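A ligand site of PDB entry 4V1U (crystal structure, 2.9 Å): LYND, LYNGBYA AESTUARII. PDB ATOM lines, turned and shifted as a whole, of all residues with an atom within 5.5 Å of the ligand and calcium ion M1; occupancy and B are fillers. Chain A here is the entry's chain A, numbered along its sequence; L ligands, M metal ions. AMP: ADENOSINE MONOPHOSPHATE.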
ATOM      1  N   ARG A 344      -4.968  17.690  17.386  1.00  0.00           N
ATOM      2  CA  ARG A 344      -3.922  17.039  18.149  1.00  0.00           C
ATOM      3  C   ARG A 344      -2.556  17.343  17.557  1.00  0.00           C
ATOM      4  O   ARG A 344      -2.462  17.928  16.473  1.00  0.00           O
ATOM      5  CB  ARG A 344      -4.167  15.535  18.202  1.00  0.00           C
ATOM      6  CG  ARG A 344      -5.447  15.186  18.933  1.00  0.00           C
ATOM      7  CD  ARG A 344      -5.761  13.703  18.911  1.00  0.00           C
ATOM      8  NE  ARG A 344      -7.002  13.409  19.612  1.00  0.00           N
ATOM      9  CZ  ARG A 344      -7.145  13.421  20.936  1.00  0.00           C
ATOM     10  NH1 ARG A 344      -6.110  13.727  21.726  1.00  0.00           N
ATOM     11  NH2 ARG A 344      -8.316  13.129  21.476  1.00  0.00           N
ATOM     12  N   THR A 346      -0.091  15.005  16.954  1.00  0.00           N
ATOM     13  CA  THR A 346       0.340  13.910  16.084  1.00  0.00           C
ATOM     14  C   THR A 346      -0.846  13.103  15.568  1.00  0.00           C
ATOM     15  O   THR A 346      -1.947  13.186  16.113  1.00  0.00           O
ATOM     16  CB  THR A 346       1.301  12.948  16.815  1.00  0.00           C
ATOM     17  OG1 THR A 346       0.798  12.675  18.130  1.00  0.00           O
ATOM     18  CG2 THR A 346       2.686  13.564  16.915  1.00  0.00           C
ATOM     19  N   THR A 347      -0.605  12.305  14.531  1.00  0.00           N
ATOM     20  CA  THR A 347      -1.653  11.516  13.900  1.00  0.00           C
ATOM     21  C   THR A 347      -2.073  10.377  14.806  1.00  0.00           C
ATOM     22  O   THR A 347      -1.344  10.024  15.738  1.00  0.00           O
ATOM     23  CB  THR A 347      -1.193  10.943  12.546  1.00  0.00           C
ATOM     24  OG1 THR A 347      -0.125  10.008  12.753  1.00  0.00           O
ATOM     25  CG2 THR A 347      -0.710  12.064  11.634  1.00  0.00           C
ATOM     26  N   PRO A 348      -3.240   9.787  14.545  1.00  0.00           N
ATOM     27  CA  PRO A 348      -3.640   8.614  15.322  1.00  0.00           C
ATOM     28  C   PRO A 348      -2.732   7.403  15.100  1.00  0.00           C
ATOM     29  O   PRO A 348      -2.337   6.770  16.067  1.00  0.00           O
ATOM     30  CB  PRO A 348      -5.057   8.314  14.825  1.00  0.00           C
ATOM     31  CG  PRO A 348      -5.196   9.045  13.549  1.00  0.00           C
ATOM     32  CD  PRO A 348      -4.325  10.249  13.672  1.00  0.00           C
ATOM     33  N   THR A 351       0.170   7.617  17.052  1.00  0.00           N
ATOM     34  CA  THR A 351      -0.200   7.380  18.442  1.00  0.00           C
ATOM     35  C   THR A 351      -0.418   5.890  18.675  1.00  0.00           C
ATOM     36  O   THR A 351       0.003   5.351  19.705  1.00  0.00           O
ATOM     37  CB  THR A 351      -1.489   8.152  18.835  1.00  0.00           C
ATOM     38  OG1 THR A 351      -1.256   9.559  18.736  1.00  0.00           O
ATOM     39  CG2 THR A 351      -1.886   7.842  20.252  1.00  0.00           C
ATOM     40  N   SER A 407     -14.381   1.683  24.346  1.00  0.00           N
ATOM     41  CA  SER A 407     -14.894   1.713  22.997  1.00  0.00           C
ATOM     42  C   SER A 407     -14.328   2.866  22.194  1.00  0.00           C
ATOM     43  O   SER A 407     -14.160   3.972  22.712  1.00  0.00           O
ATOM     44  CB  SER A 407     -16.410   1.782  23.004  1.00  0.00           C
ATOM     45  OG  SER A 407     -16.915   1.522  21.713  1.00  0.00           O
ATOM     46  N   GLY A 408     -14.041   2.608  20.931  1.00  0.00           N
ATOM     47  CA  GLY A 408     -13.467   3.587  20.040  1.00  0.00           C
ATOM     48  C   GLY A 408     -14.477   4.091  19.041  1.00  0.00           C
ATOM     49  O   GLY A 408     -15.188   3.289  18.425  1.00  0.00           O
ATOM     50  N   LYS A 409     -14.561   5.404  18.898  1.00  0.00           N
ATOM     51  CA  LYS A 409     -15.474   6.038  17.954  1.00  0.00           C
ATOM     52  C   LYS A 409     -14.667   6.935  17.018  1.00  0.00           C
ATOM     53  O   LYS A 409     -13.633   7.481  17.414  1.00  0.00           O
ATOM     54  CB  LYS A 409     -16.549   6.839  18.691  1.00  0.00           C
ATOM     55  CG  LYS A 409     -15.992   7.977  19.524  1.00  0.00           C
ATOM     56  CD  LYS A 409     -17.074   8.816  20.196  1.00  0.00           C
ATOM     57  CE  LYS A 409     -16.488   9.843  21.162  1.00  0.00           C
ATOM     58  NZ  LYS A 409     -15.601  10.825  20.484  1.00  0.00           N
ATOM     59  N   GLN A 415      -8.489   6.670  13.525  1.00  0.00           N
ATOM     60  CA  GLN A 415      -8.888   7.504  14.658  1.00  0.00           C
ATOM     61  C   GLN A 415      -9.822   6.744  15.592  1.00  0.00           C
ATOM     62  O   GLN A 415      -9.813   6.957  16.809  1.00  0.00           O
ATOM     63  CB  GLN A 415      -9.526   8.806  14.183  1.00  0.00           C
ATOM     64  CG  GLN A 415     -10.178   9.639  15.289  1.00  0.00           C
ATOM     65  CD  GLN A 415      -9.238   9.923  16.466  1.00  0.00           C
ATOM     66  OE1 GLN A 415      -8.020   9.930  16.311  1.00  0.00           O
ATOM     67  NE2 GLN A 415      -9.815  10.159  17.645  1.00  0.00           N
ATOM     68  N   ALA A 418      -7.333   4.570  17.612  1.00  0.00           N
ATOM     69  CA  ALA A 418      -6.648   5.359  18.633  1.00  0.00           C
ATOM     70  C   ALA A 418      -7.571   5.677  19.789  1.00  0.00           C
ATOM     71  O   ALA A 418      -7.146   5.742  20.939  1.00  0.00           O
ATOM     72  CB  ALA A 418      -6.126   6.639  18.026  1.00  0.00           C
ATOM     73  N   SER A 419      -8.846   5.880  19.472  1.00  0.00           N
ATOM     74  CA  SER A 419      -9.844   6.199  20.470  1.00  0.00           C
ATOM     75  C   SER A 419     -10.034   5.032  21.437  1.00  0.00           C
ATOM     76  O   SER A 419     -10.015   5.204  22.648  1.00  0.00           O
ATOM     77  CB  SER A 419     -11.166   6.532  19.791  1.00  0.00           C
ATOM     78  OG  SER A 419     -12.177   6.819  20.744  1.00  0.00           O
ATOM     79  N   CYS A 422      -6.756   4.402  23.593  1.00  0.00           N
ATOM     80  CA  CYS A 422      -6.380   5.430  24.548  1.00  0.00           C
ATOM     81  C   CYS A 422      -7.428   5.611  25.635  1.00  0.00           C
ATOM     82  O   CYS A 422      -7.129   6.158  26.679  1.00  0.00           O
ATOM     83  CB  CYS A 422      -6.129   6.761  23.836  1.00  0.00           C
ATOM     84  SG  CYS A 422      -4.650   6.752  22.787  1.00  0.00           S
ATOM     85  N   GLU A 423      -8.647   5.147  25.381  1.00  0.00           N
ATOM     86  CA  GLU A 423      -9.685   5.203  26.413  1.00  0.00           C
ATOM     87  C   GLU A 423      -9.412   4.126  27.451  1.00  0.00           C
ATOM     88  O   GLU A 423      -9.613   4.338  28.643  1.00  0.00           O
ATOM     89  CB  GLU A 423     -11.082   5.013  25.824  1.00  0.00           C
ATOM     90  CG  GLU A 423     -12.210   5.141  26.849  1.00  0.00           C
ATOM     91  CD  GLU A 423     -12.306   6.520  27.458  1.00  0.00           C
ATOM     92  OE1 GLU A 423     -11.693   7.469  26.923  1.00  0.00           O
ATOM     93  OE2 GLU A 423     -13.004   6.674  28.484  1.00  0.00           O
ATOM     94  N   GLU A 426      -6.541   5.350  29.591  1.00  0.00           N
ATOM     95  CA  GLU A 426      -7.051   6.413  30.446  1.00  0.00           C
ATOM     96  C   GLU A 426      -7.645   5.799  31.690  1.00  0.00           C
ATOM     97  O   GLU A 426      -7.410   6.271  32.794  1.00  0.00           O
ATOM     98  CB  GLU A 426      -8.088   7.267  29.686  1.00  0.00           C
ATOM     99  CG  GLU A 426      -9.199   7.897  30.542  1.00  0.00           C
ATOM    100  CD  GLU A 426     -10.311   8.528  29.705  1.00  0.00           C
ATOM    101  OE1 GLU A 426     -10.021   9.052  28.613  1.00  0.00           O
ATOM    102  OE2 GLU A 426     -11.482   8.496  30.136  1.00  0.00           O
ATOM    103  N   SER A 529     -15.592   9.020  36.241  1.00  0.00           N
ATOM    104  CA  SER A 529     -14.849   9.164  34.994  1.00  0.00           C
ATOM    105  C   SER A 529     -14.950  10.579  34.417  1.00  0.00           C
ATOM    106  O   SER A 529     -14.561  10.820  33.273  1.00  0.00           O
ATOM    107  CB  SER A 529     -15.390   8.167  33.975  1.00  0.00           C
ATOM    108  OG  SER A 529     -16.796   8.275  33.897  1.00  0.00           O
ATOM    109  N   ASN A 532     -11.783  12.906  32.951  1.00  0.00           N
ATOM    110  CA  ASN A 532     -10.611  12.096  32.649  1.00  0.00           C
ATOM    111  C   ASN A 532     -10.328  12.100  31.153  1.00  0.00           C
ATOM    112  O   ASN A 532     -11.255  12.014  30.343  1.00  0.00           O
ATOM    113  CB  ASN A 532     -10.819  10.649  33.120  1.00  0.00           C
ATOM    114  CG  ASN A 532     -10.898  10.516  34.630  1.00  0.00           C
ATOM    115  OD1 ASN A 532     -11.628  11.254  35.285  1.00  0.00           O
ATOM    116  ND2 ASN A 532     -10.142   9.561  35.176  1.00  0.00           N
ATOM    117  N   ALA A 533      -9.055  12.213  30.794  1.00  0.00           N
ATOM    118  CA  ALA A 533      -8.655  12.232  29.384  1.00  0.00           C
ATOM    119  C   ALA A 533      -7.192  11.864  29.171  1.00  0.00           C
ATOM    120  O   ALA A 533      -6.325  12.264  29.943  1.00  0.00           O
ATOM    121  CB  ALA A 533      -8.925  13.595  28.796  1.00  0.00           C
ATOM    122  N   ALA A 534      -6.929  11.099  28.114  1.00  0.00           N
ATOM    123  CA  ALA A 534      -5.561  10.822  27.694  1.00  0.00           C
ATOM    124  C   ALA A 534      -5.171  11.704  26.504  1.00  0.00           C
ATOM    125  O   ALA A 534      -6.010  12.403  25.929  1.00  0.00           O
ATOM    126  CB  ALA A 534      -5.388   9.360  27.346  1.00  0.00           C
ATOM    127  N   GLY A 535      -3.892  11.672  26.144  1.00  0.00           N
ATOM    128  CA  GLY A 535      -3.378  12.476  25.044  1.00  0.00           C
ATOM    129  C   GLY A 535      -1.885  12.282  24.872  1.00  0.00           C
ATOM    130  O   GLY A 535      -1.207  11.784  25.770  1.00  0.00           O
ATOM    131  N   ASN A 536      -1.374  12.684  23.706  1.00  0.00           N
ATOM    132  CA  ASN A 536       0.057  12.549  23.437  1.00  0.00           C
ATOM    133  C   ASN A 536       0.886  13.562  24.223  1.00  0.00           C
ATOM    134  O   ASN A 536       2.092  13.359  24.419  1.00  0.00           O
ATOM    135  CB  ASN A 536       0.311  12.673  21.944  1.00  0.00           C
ATOM    136  CG  ASN A 536      -0.378  11.596  21.146  1.00  0.00           C
ATOM    137  OD1 ASN A 536       0.045  10.436  21.149  1.00  0.00           O
ATOM    138  ND2 ASN A 536      -1.455  11.970  20.442  1.00  0.00           N
ATOM    139  N   GLU A 540      -2.593  18.580  25.502  1.00  0.00           N
ATOM    140  CA  GLU A 540      -3.545  17.874  24.667  1.00  0.00           C
ATOM    141  C   GLU A 540      -4.593  17.176  25.522  1.00  0.00           C
ATOM    142  O   GLU A 540      -5.786  17.189  25.212  1.00  0.00           O
ATOM    143  CB  GLU A 540      -2.822  16.865  23.783  1.00  0.00           C
ATOM    144  CG  GLU A 540      -3.698  16.176  22.748  1.00  0.00           C
ATOM    145  CD  GLU A 540      -2.895  15.467  21.666  1.00  0.00           C
ATOM    146  OE1 GLU A 540      -1.949  16.092  21.114  1.00  0.00           O
ATOM    147  OE2 GLU A 540      -3.208  14.300  21.358  1.00  0.00           O
ATOM    148  N   GLN A 544      -8.834  18.084  26.169  1.00  0.00           N
ATOM    149  CA  GLN A 544      -9.915  17.137  25.913  1.00  0.00           C
ATOM    150  C   GLN A 544     -10.723  16.897  27.174  1.00  0.00           C
ATOM    151  O   GLN A 544     -11.941  16.738  27.114  1.00  0.00           O
ATOM    152  CB  GLN A 544      -9.375  15.808  25.395  1.00  0.00           C
ATOM    153  CG  GLN A 544     -10.425  14.977  24.671  1.00  0.00           C
ATOM    154  CD  GLN A 544     -10.551  15.353  23.198  1.00  0.00           C
ATOM    155  OE1 GLN A 544      -9.950  16.314  22.725  1.00  0.00           O
ATOM    156  NE2 GLN A 544     -11.335  14.571  22.457  1.00  0.00           N
ATOM    157  N   GLU A 548     -14.842  17.316  28.101  1.00  0.00           N
ATOM    158  CA  GLU A 548     -15.717  16.275  28.640  1.00  0.00           C
ATOM    159  C   GLU A 548     -16.647  16.882  29.680  1.00  0.00           C
ATOM    160  O   GLU A 548     -17.818  16.539  29.739  1.00  0.00           O
ATOM    161  CB  GLU A 548     -14.903  15.129  29.257  1.00  0.00           C
ATOM    162  CG  GLU A 548     -14.061  14.336  28.275  1.00  0.00           C
ATOM    163  CD  GLU A 548     -14.890  13.431  27.359  1.00  0.00           C
ATOM    164  OE1 GLU A 548     -15.853  12.799  27.846  1.00  0.00           O
ATOM    165  OE2 GLU A 548     -14.560  13.351  26.151  1.00  0.00           O
ATOM    166  N   ARG A 552     -20.977  17.080  29.614  1.00  0.00           N
ATOM    167  CA  ARG A 552     -21.786  16.479  30.664  1.00  0.00           C
ATOM    168  C   ARG A 552     -22.614  17.560  31.360  1.00  0.00           C
ATOM    169  O   ARG A 552     -23.711  17.299  31.864  1.00  0.00           O
ATOM    170  CB  ARG A 552     -20.912  15.751  31.696  1.00  0.00           C
ATOM    171  CG  ARG A 552     -19.803  14.914  31.098  1.00  0.00           C
ATOM    172  CD  ARG A 552     -19.934  13.445  31.385  1.00  0.00           C
ATOM    173  NE  ARG A 552     -19.375  12.665  30.283  1.00  0.00           N
ATOM    174  CZ  ARG A 552     -18.700  11.529  30.417  1.00  0.00           C
ATOM    175  NH1 ARG A 552     -18.455  11.005  31.611  1.00  0.00           N
ATOM    176  NH2 ARG A 552     -18.255  10.922  29.315  1.00  0.00           N
ATOM    177  N   ARG A 636     -17.849  14.229  17.048  1.00  0.00           N
ATOM    178  CA  ARG A 636     -17.764  13.482  18.308  1.00  0.00           C
ATOM    179  C   ARG A 636     -19.115  12.899  18.711  1.00  0.00           C
ATOM    180  O   ARG A 636     -19.198  11.779  19.200  1.00  0.00           O
ATOM    181  CB  ARG A 636     -17.208  14.375  19.414  1.00  0.00           C
ATOM    182  CG  ARG A 636     -15.716  14.628  19.319  1.00  0.00           C
ATOM    183  CD  ARG A 636     -15.194  15.406  20.517  1.00  0.00           C
ATOM    184  NE  ARG A 636     -15.266  14.618  21.751  1.00  0.00           N
ATOM    185  CZ  ARG A 636     -14.481  13.580  22.027  1.00  0.00           C
ATOM    186  NH1 ARG A 636     -13.550  13.189  21.161  1.00  0.00           N
ATOM    187  NH2 ARG A 636     -14.634  12.932  23.176  1.00  0.00           N
ATOM    188  N   LEU A 727       1.886   7.464  27.894  1.00  0.00           N
ATOM    189  CA  LEU A 727       0.741   8.269  27.461  1.00  0.00           C
ATOM    190  C   LEU A 727       0.223   9.111  28.612  1.00  0.00           C
ATOM    191  O   LEU A 727      -0.016   8.619  29.702  1.00  0.00           O
ATOM    192  CB  LEU A 727      -0.376   7.359  26.927  1.00  0.00           C
ATOM    193  CG  LEU A 727      -1.576   8.060  26.265  1.00  0.00           C
ATOM    194  CD1 LEU A 727      -1.157   8.799  25.011  1.00  0.00           C
ATOM    195  CD2 LEU A 727      -2.669   7.053  25.933  1.00  0.00           C
HETATM  196  P   AMP L   1     -13.093   9.734  22.646  1.00  0.00           P
HETATM  197  O1P AMP L   1     -13.714   8.381  22.392  1.00  0.00           O
HETATM  198  O2P AMP L   1     -13.720  10.487  23.791  1.00  0.00           O
HETATM  199  O3P AMP L   1     -12.809  10.575  21.426  1.00  0.00           O
HETATM  200  O5' AMP L   1     -11.611   9.403  23.114  1.00  0.00           O
HETATM  201  C5' AMP L   1     -11.377   8.620  24.285  1.00  0.00           C
HETATM  202  C4' AMP L   1     -10.020   8.916  24.880  1.00  0.00           C
HETATM  203  O4' AMP L   1      -9.029   8.657  23.877  1.00  0.00           O
HETATM  204  C3' AMP L   1      -9.832  10.376  25.316  1.00  0.00           C
HETATM  205  O3' AMP L   1      -9.069  10.423  26.511  1.00  0.00           O
HETATM  206  C2' AMP L   1      -9.033  10.998  24.181  1.00  0.00           C
HETATM  207  O2' AMP L   1      -8.226  12.099  24.572  1.00  0.00           O
HETATM  208  C1' AMP L   1      -8.201   9.810  23.709  1.00  0.00           C
HETATM  209  N9  AMP L   1      -7.803   9.901  22.299  1.00  0.00           N
HETATM  210  C8  AMP L   1      -8.617   9.776  21.238  1.00  0.00           C
HETATM  211  N7  AMP L   1      -7.903   9.936  20.094  1.00  0.00           N
HETATM  212  C5  AMP L   1      -6.618  10.170  20.427  1.00  0.00           C
HETATM  213  C6  AMP L   1      -5.337  10.420  19.723  1.00  0.00           C
HETATM  214  N6  AMP L   1      -5.298  10.452  18.375  1.00  0.00           N
HETATM  215  N1  AMP L   1      -4.229  10.608  20.470  1.00  0.00           N
HETATM  216  C2  AMP L   1      -4.251  10.570  21.821  1.00  0.00           C
HETATM  217  N3  AMP L   1      -5.372  10.347  22.525  1.00  0.00           N
HETATM  218  C4  AMP L   1      -6.560  10.145  21.897  1.00  0.00           C
HETATM  219 CA    CA M   1     -13.166   9.495  28.558  1.00  0.00          CA
HETATM  220 CA    CA M   2     -17.715  10.120  24.687  1.00  0.00          CA
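OE1 of Glu 426 sits at hydrogen-bond distance from O3' of the ligand (2.7 Å). N3 of the ligand sits at hydrogen-bond distance from SG of Cys 422 (3.7 Å). O1P of the ligand is in hydrogen-bond range of OG of Ser 419, 2.7 Å away. An oxygen (O2') of the ligand lies within hydrogen-bond range of the guanidinium group (NH2) of Arg 344, 3.3 Å away. The backbone carbonyl oxygen (O) of Ala 534 lies within hydrogen-bond range of an oxygen (O2') of the ligand, 2.6 Å away. NE2 of Gln 415 sits at hydrogen-bond distance from N7 of the ligand, at 3.1 Å. NZ of Lys 409 lies within salt-bridge range of O3P of the ligand (3.0 Å). The guanidinium group of Arg 636 is in salt-bridge range of an oxygen (O2P) of the ligand (2.7 Å). N of Ala 534 sits at hydrogen-bond distance from O3' of the ligand (2.8 Å). The side-chain amide nitrogen (ND2) of Asn 536 lies within hydrogen-bond range of a nitrogen (N1) of the ligand, 3.1 Å away.
The side-chain carboxylate (OE1) of Glu 548 is in salt-bridge range of the guanidinium group (NH2) of Arg 552. OG1 of Thr 351 is in hydrogen-bond range of O of Thr 347, 3.0 Å away. The side-chain hydroxyl (OG) of Ser 419 is in hydrogen-bond range of the backbone NH (N) of Lys 409. The side-chain hydroxyl (OG1) of Thr 351 is in hydrogen-bond range of the side-chain amide oxygen (OD1) of Asn 536 (2.9 Å). The guanidinium group (NH1) of Arg 344 is in salt-bridge range of the side-chain carboxylate (OE2) of Glu 540, 3.0 Å away. The guanidinium group of Arg 636 is in salt-bridge range of the side-chain carboxylate of Glu 548. NE2 of Gln 544 lies close to NH1 of Arg 636, at 2.9 Å. The backbone carbonyl oxygen of Ala 418 sits close to the side-chain sulfur of Cys 422.
Residues that only touch the ligand: Ala 533 (3.4 Å), Thr 351 (3.6 Å), Gln 544 (3.6 Å), Glu 548 (3.8 Å), Gly 535 (3.8 Å), Glu 540 (3.9 Å), Ala 418 (3.9 Å) and Pro 348 (3.9 Å). Hydrophobic or aromatic side chains that line the ligand: Ala 418, Ala 533 and Ala 534. 18 residues have an atom within 4 Å of the ligand: Arg 344, Pro 348, Thr 351, Lys 409, Gln 415, Ala 418, Ser 419, Cys 422, Glu 423, Glu 426, Ala 533, Ala 534, Gly 535, Asn 536, Glu 540, Gln 544, Glu 548 and Arg 636.
Asn 532 touches calcium ion M1. Within 4 Å of calcium ion M1: Glu 423, Glu 426 and Asn 532. The nearest printed residue that does not touch calcium ion M1 is Glu 548 (4.3 Å).
Calcium ion M1 is bound by the side-chain carboxylate of Glu 426 and the side-chain carboxylate of Glu 423. Calcium ion M1 has two donor atoms within binding distance. Slightly farther from calcium ion M1 lies OE1 of Glu 423 (3.0 Å).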
